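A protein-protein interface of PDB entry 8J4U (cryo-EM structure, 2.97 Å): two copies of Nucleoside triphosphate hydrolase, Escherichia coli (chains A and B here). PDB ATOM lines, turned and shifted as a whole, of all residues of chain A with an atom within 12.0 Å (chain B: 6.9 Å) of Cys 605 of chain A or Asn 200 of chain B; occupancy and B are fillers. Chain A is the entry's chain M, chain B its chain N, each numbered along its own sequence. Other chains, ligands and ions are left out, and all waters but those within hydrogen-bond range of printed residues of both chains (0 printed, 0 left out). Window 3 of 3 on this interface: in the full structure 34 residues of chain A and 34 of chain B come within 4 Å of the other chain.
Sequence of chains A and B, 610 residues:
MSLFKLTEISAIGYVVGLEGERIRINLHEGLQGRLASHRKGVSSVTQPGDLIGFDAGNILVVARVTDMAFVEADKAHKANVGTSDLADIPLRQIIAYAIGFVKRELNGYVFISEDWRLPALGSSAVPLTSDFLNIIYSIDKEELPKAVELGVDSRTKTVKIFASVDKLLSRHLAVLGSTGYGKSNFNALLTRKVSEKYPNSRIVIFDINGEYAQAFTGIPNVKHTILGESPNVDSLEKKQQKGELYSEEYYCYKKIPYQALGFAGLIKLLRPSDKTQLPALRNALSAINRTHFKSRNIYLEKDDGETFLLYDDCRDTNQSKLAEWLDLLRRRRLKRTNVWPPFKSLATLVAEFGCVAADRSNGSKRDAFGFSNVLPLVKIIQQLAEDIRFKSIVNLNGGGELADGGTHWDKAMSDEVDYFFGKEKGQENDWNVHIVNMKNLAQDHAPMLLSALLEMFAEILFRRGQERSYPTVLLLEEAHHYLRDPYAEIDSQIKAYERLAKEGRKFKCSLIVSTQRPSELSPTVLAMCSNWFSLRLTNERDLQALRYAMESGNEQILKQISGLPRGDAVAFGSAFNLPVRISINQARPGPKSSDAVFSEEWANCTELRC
Printed residues of chain B within 4 Å of Phe 598 of chain A: Pro 471 (3.9 Å).
Of chain B, only Asn 200 (3.3 Å) comes within 4 Å of Cys 605 of chain A.
No residue of chain A comes within 4 Å of Pro 199 of chain B.
Of the printed residues of chain A, Asn 200 of chain B touches Trp 602 (3.3 Å) and Cys 605 (3.3 Å).
No residue of chain A comes within 4 Å of Asn 432 of chain B.
Of the printed residues of chain A, Pro 471 of chain B touches Phe 598 (3.9 Å) and Trp 602 (3.5 Å).
The nearest residue of chain B that does not touch Cys 605 of chain A is Tyr 470 of chain B (4.6 Å).
No position is printed for both chains.
Among the printed residues, pairs that only touch across the chains: Phe 598 of chain A with Pro 471 of chain B (3.9 Å), Ser 599 of chain A with Tyr 198 of chain B (3.6 Å), Glu 601 of chain A with Tyr 470 of chain B (3.7 Å), Trp 602 of chain A with Asn 200 of chain B (3.3 Å), Trp 602 of chain A with Ser 201 of chain B (3.98 Å), Trp 602 of chain A with Tyr 470 of chain B (3.6 Å), Trp 602 of chain A with Pro 471 of chain B (3.5 Å) and Cys 605 of chain A with Asn 200 of chain B (3.3 Å).
OD1 of Asn 432 of chain B lies close to O of Ser 201 of chain B (2.6 Å).
The backbone carbonyl oxygen (O) of Tyr 198 of chain B sits at hydrogen-bond distance from the side-chain hydroxyl (OG) of Ser 201 of chain B, 2.8 Å away.
Hydrophobic or aromatic side chains of chain B that line the printed part of chain A: Tyr 198, Tyr 470 and Pro 471.
Hydrophobic or aromatic side chains of chain A within 4 Å of the printed part of chain B: Phe 598 and Trp 602.
Along chain A the printed residues that touch a printed residue of chain B span positions 598 to 605.
Among the printed residues, no Asp or Glu carboxylate lies within 4 Å of a Lys or Arg side-chain nitrogen of the other chain.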
ATOM      1  N   VAL A 597      29.602   8.463  -7.755  1.00  0.00           N
ATOM      2  CA  VAL A 597      29.818   7.967  -9.106  1.00  0.00           C
ATOM      3  C   VAL A 597      28.520   7.315  -9.586  1.00  0.00           C
ATOM      4  O   VAL A 597      27.611   7.044  -8.801  1.00  0.00           O
ATOM      5  CB  VAL A 597      31.006   6.984  -9.179  1.00  0.00           C
ATOM      6  CG1 VAL A 597      31.338   6.629 -10.614  1.00  0.00           C
ATOM      7  CG2 VAL A 597      32.224   7.578  -8.492  1.00  0.00           C
ATOM      8  N   PHE A 598      28.445   7.062 -10.894  1.00  0.00           N
ATOM      9  CA  PHE A 598      27.208   6.641 -11.538  1.00  0.00           C
ATOM     10  C   PHE A 598      27.249   5.243 -12.132  1.00  0.00           C
ATOM     11  O   PHE A 598      26.228   4.552 -12.104  1.00  0.00           O
ATOM     12  CB  PHE A 598      26.842   7.620 -12.664  1.00  0.00           C
ATOM     13  CG  PHE A 598      26.031   8.797 -12.209  1.00  0.00           C
ATOM     14  CD1 PHE A 598      24.886   9.168 -12.890  1.00  0.00           C
ATOM     15  CD2 PHE A 598      26.419   9.540 -11.112  1.00  0.00           C
ATOM     16  CE1 PHE A 598      24.142  10.251 -12.479  1.00  0.00           C
ATOM     17  CE2 PHE A 598      25.676  10.626 -10.697  1.00  0.00           C
ATOM     18  CZ  PHE A 598      24.538  10.980 -11.382  1.00  0.00           C
ATOM     19  N   SER A 599      28.387   4.803 -12.669  1.00  0.00           N
ATOM     20  CA  SER A 599      28.423   3.527 -13.378  1.00  0.00           C
ATOM     21  C   SER A 599      28.383   2.345 -12.417  1.00  0.00           C
ATOM     22  O   SER A 599      27.753   1.323 -12.715  1.00  0.00           O
ATOM     23  CB  SER A 599      29.675   3.453 -14.251  1.00  0.00           C
ATOM     24  OG  SER A 599      30.792   3.021 -13.496  1.00  0.00           O
ATOM     25  N   GLU A 600      29.080   2.452 -11.287  1.00  0.00           N
ATOM     26  CA  GLU A 600      29.055   1.398 -10.280  1.00  0.00           C
ATOM     27  C   GLU A 600      27.627   1.085  -9.847  1.00  0.00           C
ATOM     28  O   GLU A 600      27.160  -0.055  -9.945  1.00  0.00           O
ATOM     29  CB  GLU A 600      29.901   1.817  -9.077  1.00  0.00           C
ATOM     30  CG  GLU A 600      31.340   2.163  -9.418  1.00  0.00           C
ATOM     31  CD  GLU A 600      32.021   2.960  -8.321  1.00  0.00           C
ATOM     32  OE1 GLU A 600      33.187   2.651  -7.998  1.00  0.00           O
ATOM     33  OE2 GLU A 600      31.391   3.894  -7.784  1.00  0.00           O
ATOM     34  N   GLU A 601      26.919   2.097  -9.344  1.00  0.00           N
ATOM     35  CA  GLU A 601      25.587   1.873  -8.795  1.00  0.00           C
ATOM     36  C   GLU A 601      24.615   1.317  -9.826  1.00  0.00           C
ATOM     37  O   GLU A 601      23.602   0.720  -9.446  1.00  0.00           O
ATOM     38  CB  GLU A 601      25.037   3.173  -8.210  1.00  0.00           C
ATOM     39  CG  GLU A 601      26.046   3.948  -7.376  1.00  0.00           C
ATOM     40  CD  GLU A 601      25.397   4.812  -6.312  1.00  0.00           C
ATOM     41  OE1 GLU A 601      24.295   4.461  -5.842  1.00  0.00           O
ATOM     42  OE2 GLU A 601      25.994   5.845  -5.941  1.00  0.00           O
ATOM     43  N   TRP A 602      24.894   1.493 -11.118  1.00  0.00           N
ATOM     44  CA  TRP A 602      24.015   0.998 -12.166  1.00  0.00           C
ATOM     45  C   TRP A 602      24.423  -0.367 -12.700  1.00  0.00           C
ATOM     46  O   TRP A 602      23.568  -1.090 -13.220  1.00  0.00           O
ATOM     47  CB  TRP A 602      23.970   1.989 -13.335  1.00  0.00           C
ATOM     48  CG  TRP A 602      23.180   3.229 -13.058  1.00  0.00           C
ATOM     49  CD1 TRP A 602      22.352   3.458 -11.998  1.00  0.00           C
ATOM     50  CD2 TRP A 602      23.141   4.413 -13.860  1.00  0.00           C
ATOM     51  NE1 TRP A 602      21.802   4.711 -12.091  1.00  0.00           N
ATOM     52  CE2 TRP A 602      22.271   5.318 -13.225  1.00  0.00           C
ATOM     53  CE3 TRP A 602      23.758   4.797 -15.053  1.00  0.00           C
ATOM     54  CZ2 TRP A 602      22.002   6.580 -13.741  1.00  0.00           C
ATOM     55  CZ3 TRP A 602      23.490   6.050 -15.563  1.00  0.00           C
ATOM     56  CH2 TRP A 602      22.620   6.927 -14.908  1.00  0.00           C
ATOM     57  N   ALA A 603      25.699  -0.731 -12.590  1.00  0.00           N
ATOM     58  CA  ALA A 603      26.162  -2.028 -13.064  1.00  0.00           C
ATOM     59  C   ALA A 603      26.116  -3.081 -11.963  1.00  0.00           C
ATOM     60  O   ALA A 603      25.534  -4.153 -12.151  1.00  0.00           O
ATOM     61  CB  ALA A 603      27.583  -1.907 -13.620  1.00  0.00           C
ATOM     62  N   ASN A 604      26.735  -2.790 -10.817  1.00  0.00           N
ATOM     63  CA  ASN A 604      26.709  -3.722  -9.694  1.00  0.00           C
ATOM     64  C   ASN A 604      25.289  -4.197  -9.405  1.00  0.00           C
ATOM     65  O   ASN A 604      25.042  -5.397  -9.237  1.00  0.00           O
ATOM     66  CB  ASN A 604      27.316  -3.057  -8.459  1.00  0.00           C
ATOM     67  CG  ASN A 604      28.832  -3.000  -8.514  1.00  0.00           C
ATOM     68  OD1 ASN A 604      29.445  -3.444  -9.485  1.00  0.00           O
ATOM     69  ND2 ASN A 604      29.443  -2.448  -7.474  1.00  0.00           N
ATOM     70  N   CYS A 605      24.342  -3.267  -9.343  1.00  0.00           N
ATOM     71  CA  CYS A 605      22.949  -3.606  -9.074  1.00  0.00           C
ATOM     72  C   CYS A 605      22.344  -4.388 -10.237  1.00  0.00           C
ATOM     73  O   CYS A 605      23.060  -5.022 -11.012  1.00  0.00           O
ATOM     74  CB  CYS A 605      22.127  -2.341  -8.811  1.00  0.00           C
ATOM     75  SG  CYS A 605      20.500  -2.649  -8.090  1.00  0.00           S
ATOM     76  N   SER B 195      20.575   4.086 -22.604  1.00  0.00           N
ATOM     77  CA  SER B 195      19.669   3.054 -22.112  1.00  0.00           C
ATOM     78  C   SER B 195      20.064   1.674 -22.618  1.00  0.00           C
ATOM     79  O   SER B 195      19.898   0.681 -21.902  1.00  0.00           O
ATOM     80  CB  SER B 195      18.237   3.372 -22.532  1.00  0.00           C
ATOM     81  OG  SER B 195      17.820   4.626 -22.028  1.00  0.00           O
ATOM     82  N   LYS B 197      23.089   0.676 -23.108  1.00  0.00           N
ATOM     83  CA  LYS B 197      24.355   0.280 -22.509  1.00  0.00           C
ATOM     84  C   LYS B 197      24.246   0.022 -21.012  1.00  0.00           C
ATOM     85  O   LYS B 197      24.913  -0.880 -20.496  1.00  0.00           O
ATOM     86  CB  LYS B 197      25.410   1.355 -22.772  1.00  0.00           C
ATOM     87  CG  LYS B 197      26.828   0.911 -22.505  1.00  0.00           C
ATOM     88  CD  LYS B 197      27.709   2.087 -22.138  1.00  0.00           C
ATOM     89  CE  LYS B 197      29.175   1.703 -22.135  1.00  0.00           C
ATOM     90  NZ  LYS B 197      29.607   1.174 -23.450  1.00  0.00           N
ATOM     91  N   TYR B 198      23.424   0.790 -20.298  1.00  0.00           N
ATOM     92  CA  TYR B 198      23.226   0.609 -18.861  1.00  0.00           C
ATOM     93  C   TYR B 198      21.742   0.382 -18.609  1.00  0.00           C
ATOM     94  O   TYR B 198      20.997   1.324 -18.304  1.00  0.00           O
ATOM     95  CB  TYR B 198      23.757   1.806 -18.075  1.00  0.00           C
ATOM     96  CG  TYR B 198      25.259   1.800 -17.897  1.00  0.00           C
ATOM     97  CD1 TYR B 198      25.873   0.871 -17.071  1.00  0.00           C
ATOM     98  CD2 TYR B 198      26.060   2.721 -18.556  1.00  0.00           C
ATOM     99  CE1 TYR B 198      27.243   0.860 -16.904  1.00  0.00           C
ATOM    100  CE2 TYR B 198      27.432   2.715 -18.395  1.00  0.00           C
ATOM    101  CZ  TYR B 198      28.015   1.784 -17.569  1.00  0.00           C
ATOM    102  OH  TYR B 198      29.381   1.780 -17.409  1.00  0.00           O
ATOM    103  N   PRO B 199      21.275  -0.864 -18.728  1.00  0.00           N
ATOM    104  CA  PRO B 199      19.830  -1.118 -18.615  1.00  0.00           C
ATOM    105  C   PRO B 199      19.227  -0.702 -17.286  1.00  0.00           C
ATOM    106  O   PRO B 199      18.040  -0.358 -17.242  1.00  0.00           O
ATOM    107  CB  PRO B 199      19.734  -2.634 -18.823  1.00  0.00           C
ATOM    108  CG  PRO B 199      20.921  -2.967 -19.646  1.00  0.00           C
ATOM    109  CD  PRO B 199      22.007  -2.077 -19.130  1.00  0.00           C
ATOM    110  N   ASN B 200      19.994  -0.731 -16.200  1.00  0.00           N
ATOM    111  CA  ASN B 200      19.489  -0.329 -14.895  1.00  0.00           C
ATOM    112  C   ASN B 200      19.495   1.182 -14.695  1.00  0.00           C
ATOM    113  O   ASN B 200      19.272   1.645 -13.572  1.00  0.00           O
ATOM    114  CB  ASN B 200      20.303  -1.000 -13.787  1.00  0.00           C
ATOM    115  CG  ASN B 200      19.772  -2.372 -13.418  1.00  0.00           C
ATOM    116  OD1 ASN B 200      18.645  -2.730 -13.760  1.00  0.00           O
ATOM    117  ND2 ASN B 200      20.584  -3.146 -12.713  1.00  0.00           N
ATOM    118  N   SER B 201      19.738   1.955 -15.750  1.00  0.00           N
ATOM    119  CA  SER B 201      19.730   3.403 -15.645  1.00  0.00           C
ATOM    120  C   SER B 201      18.331   3.907 -15.286  1.00  0.00           C
ATOM    121  O   SER B 201      17.343   3.173 -15.320  1.00  0.00           O
ATOM    122  CB  SER B 201      20.209   4.025 -16.954  1.00  0.00           C
ATOM    123  OG  SER B 201      19.422   3.583 -18.043  1.00  0.00           O
ATOM    124  N   ARG B 202      18.262   5.192 -14.935  1.00  0.00           N
ATOM    125  CA  ARG B 202      17.023   5.830 -14.495  1.00  0.00           C
ATOM    126  C   ARG B 202      16.914   7.178 -15.197  1.00  0.00           C
ATOM    127  O   ARG B 202      17.684   8.098 -14.901  1.00  0.00           O
ATOM    128  CB  ARG B 202      17.010   5.989 -12.975  1.00  0.00           C
ATOM    129  CG  ARG B 202      15.819   6.719 -12.398  1.00  0.00           C
ATOM    130  CD  ARG B 202      14.613   5.812 -12.292  1.00  0.00           C
ATOM    131  NE  ARG B 202      14.627   4.994 -11.082  1.00  0.00           N
ATOM    132  CZ  ARG B 202      14.519   5.472  -9.847  1.00  0.00           C
ATOM    133  NH1 ARG B 202      14.390   6.772  -9.637  1.00  0.00           N
ATOM    134  NH2 ARG B 202      14.541   4.646  -8.815  1.00  0.00           N
ATOM    135  N   ASN B 432      12.368   2.009 -15.934  1.00  0.00           N
ATOM    136  CA  ASN B 432      13.634   2.723 -15.919  1.00  0.00           C
ATOM    137  C   ASN B 432      13.622   3.971 -16.789  1.00  0.00           C
ATOM    138  O   ASN B 432      14.546   4.788 -16.683  1.00  0.00           O
ATOM    139  CB  ASN B 432      14.771   1.802 -16.387  1.00  0.00           C
ATOM    140  CG  ASN B 432      15.268   0.884 -15.292  1.00  0.00           C
ATOM    141  OD1 ASN B 432      15.782   1.336 -14.272  1.00  0.00           O
ATOM    142  ND2 ASN B 432      15.113  -0.415 -15.501  1.00  0.00           N
ATOM    143  N   TYR B 470      18.740   7.367  -5.125  1.00  0.00           N
ATOM    144  CA  TYR B 470      19.197   6.713  -6.342  1.00  0.00           C
ATOM    145  C   TYR B 470      19.486   7.751  -7.422  1.00  0.00           C
ATOM    146  O   TYR B 470      18.752   8.738  -7.541  1.00  0.00           O
ATOM    147  CB  TYR B 470      18.132   5.738  -6.842  1.00  0.00           C
ATOM    148  CG  TYR B 470      18.638   4.603  -7.702  1.00  0.00           C
ATOM    149  CD1 TYR B 470      19.631   3.747  -7.251  1.00  0.00           C
ATOM    150  CD2 TYR B 470      18.103   4.375  -8.961  1.00  0.00           C
ATOM    151  CE1 TYR B 470      20.087   2.708  -8.036  1.00  0.00           C
ATOM    152  CE2 TYR B 470      18.550   3.338  -9.750  1.00  0.00           C
ATOM    153  CZ  TYR B 470      19.540   2.508  -9.284  1.00  0.00           C
ATOM    154  OH  TYR B 470      19.985   1.475 -10.073  1.00  0.00           O
ATOM    155  N   PRO B 471      20.531   7.585  -8.236  1.00  0.00           N
ATOM    156  CA  PRO B 471      20.858   8.611  -9.232  1.00  0.00           C
ATOM    157  C   PRO B 471      20.012   8.518 -10.494  1.00  0.00           C
ATOM    158  O   PRO B 471      19.766   7.439 -11.038  1.00  0.00           O
ATOM    159  CB  PRO B 471      22.332   8.317  -9.535  1.00  0.00           C
ATOM    160  CG  PRO B 471      22.442   6.868  -9.354  1.00  0.00           C
ATOM    161  CD  PRO B 471      21.582   6.556  -8.168  1.00  0.00           C
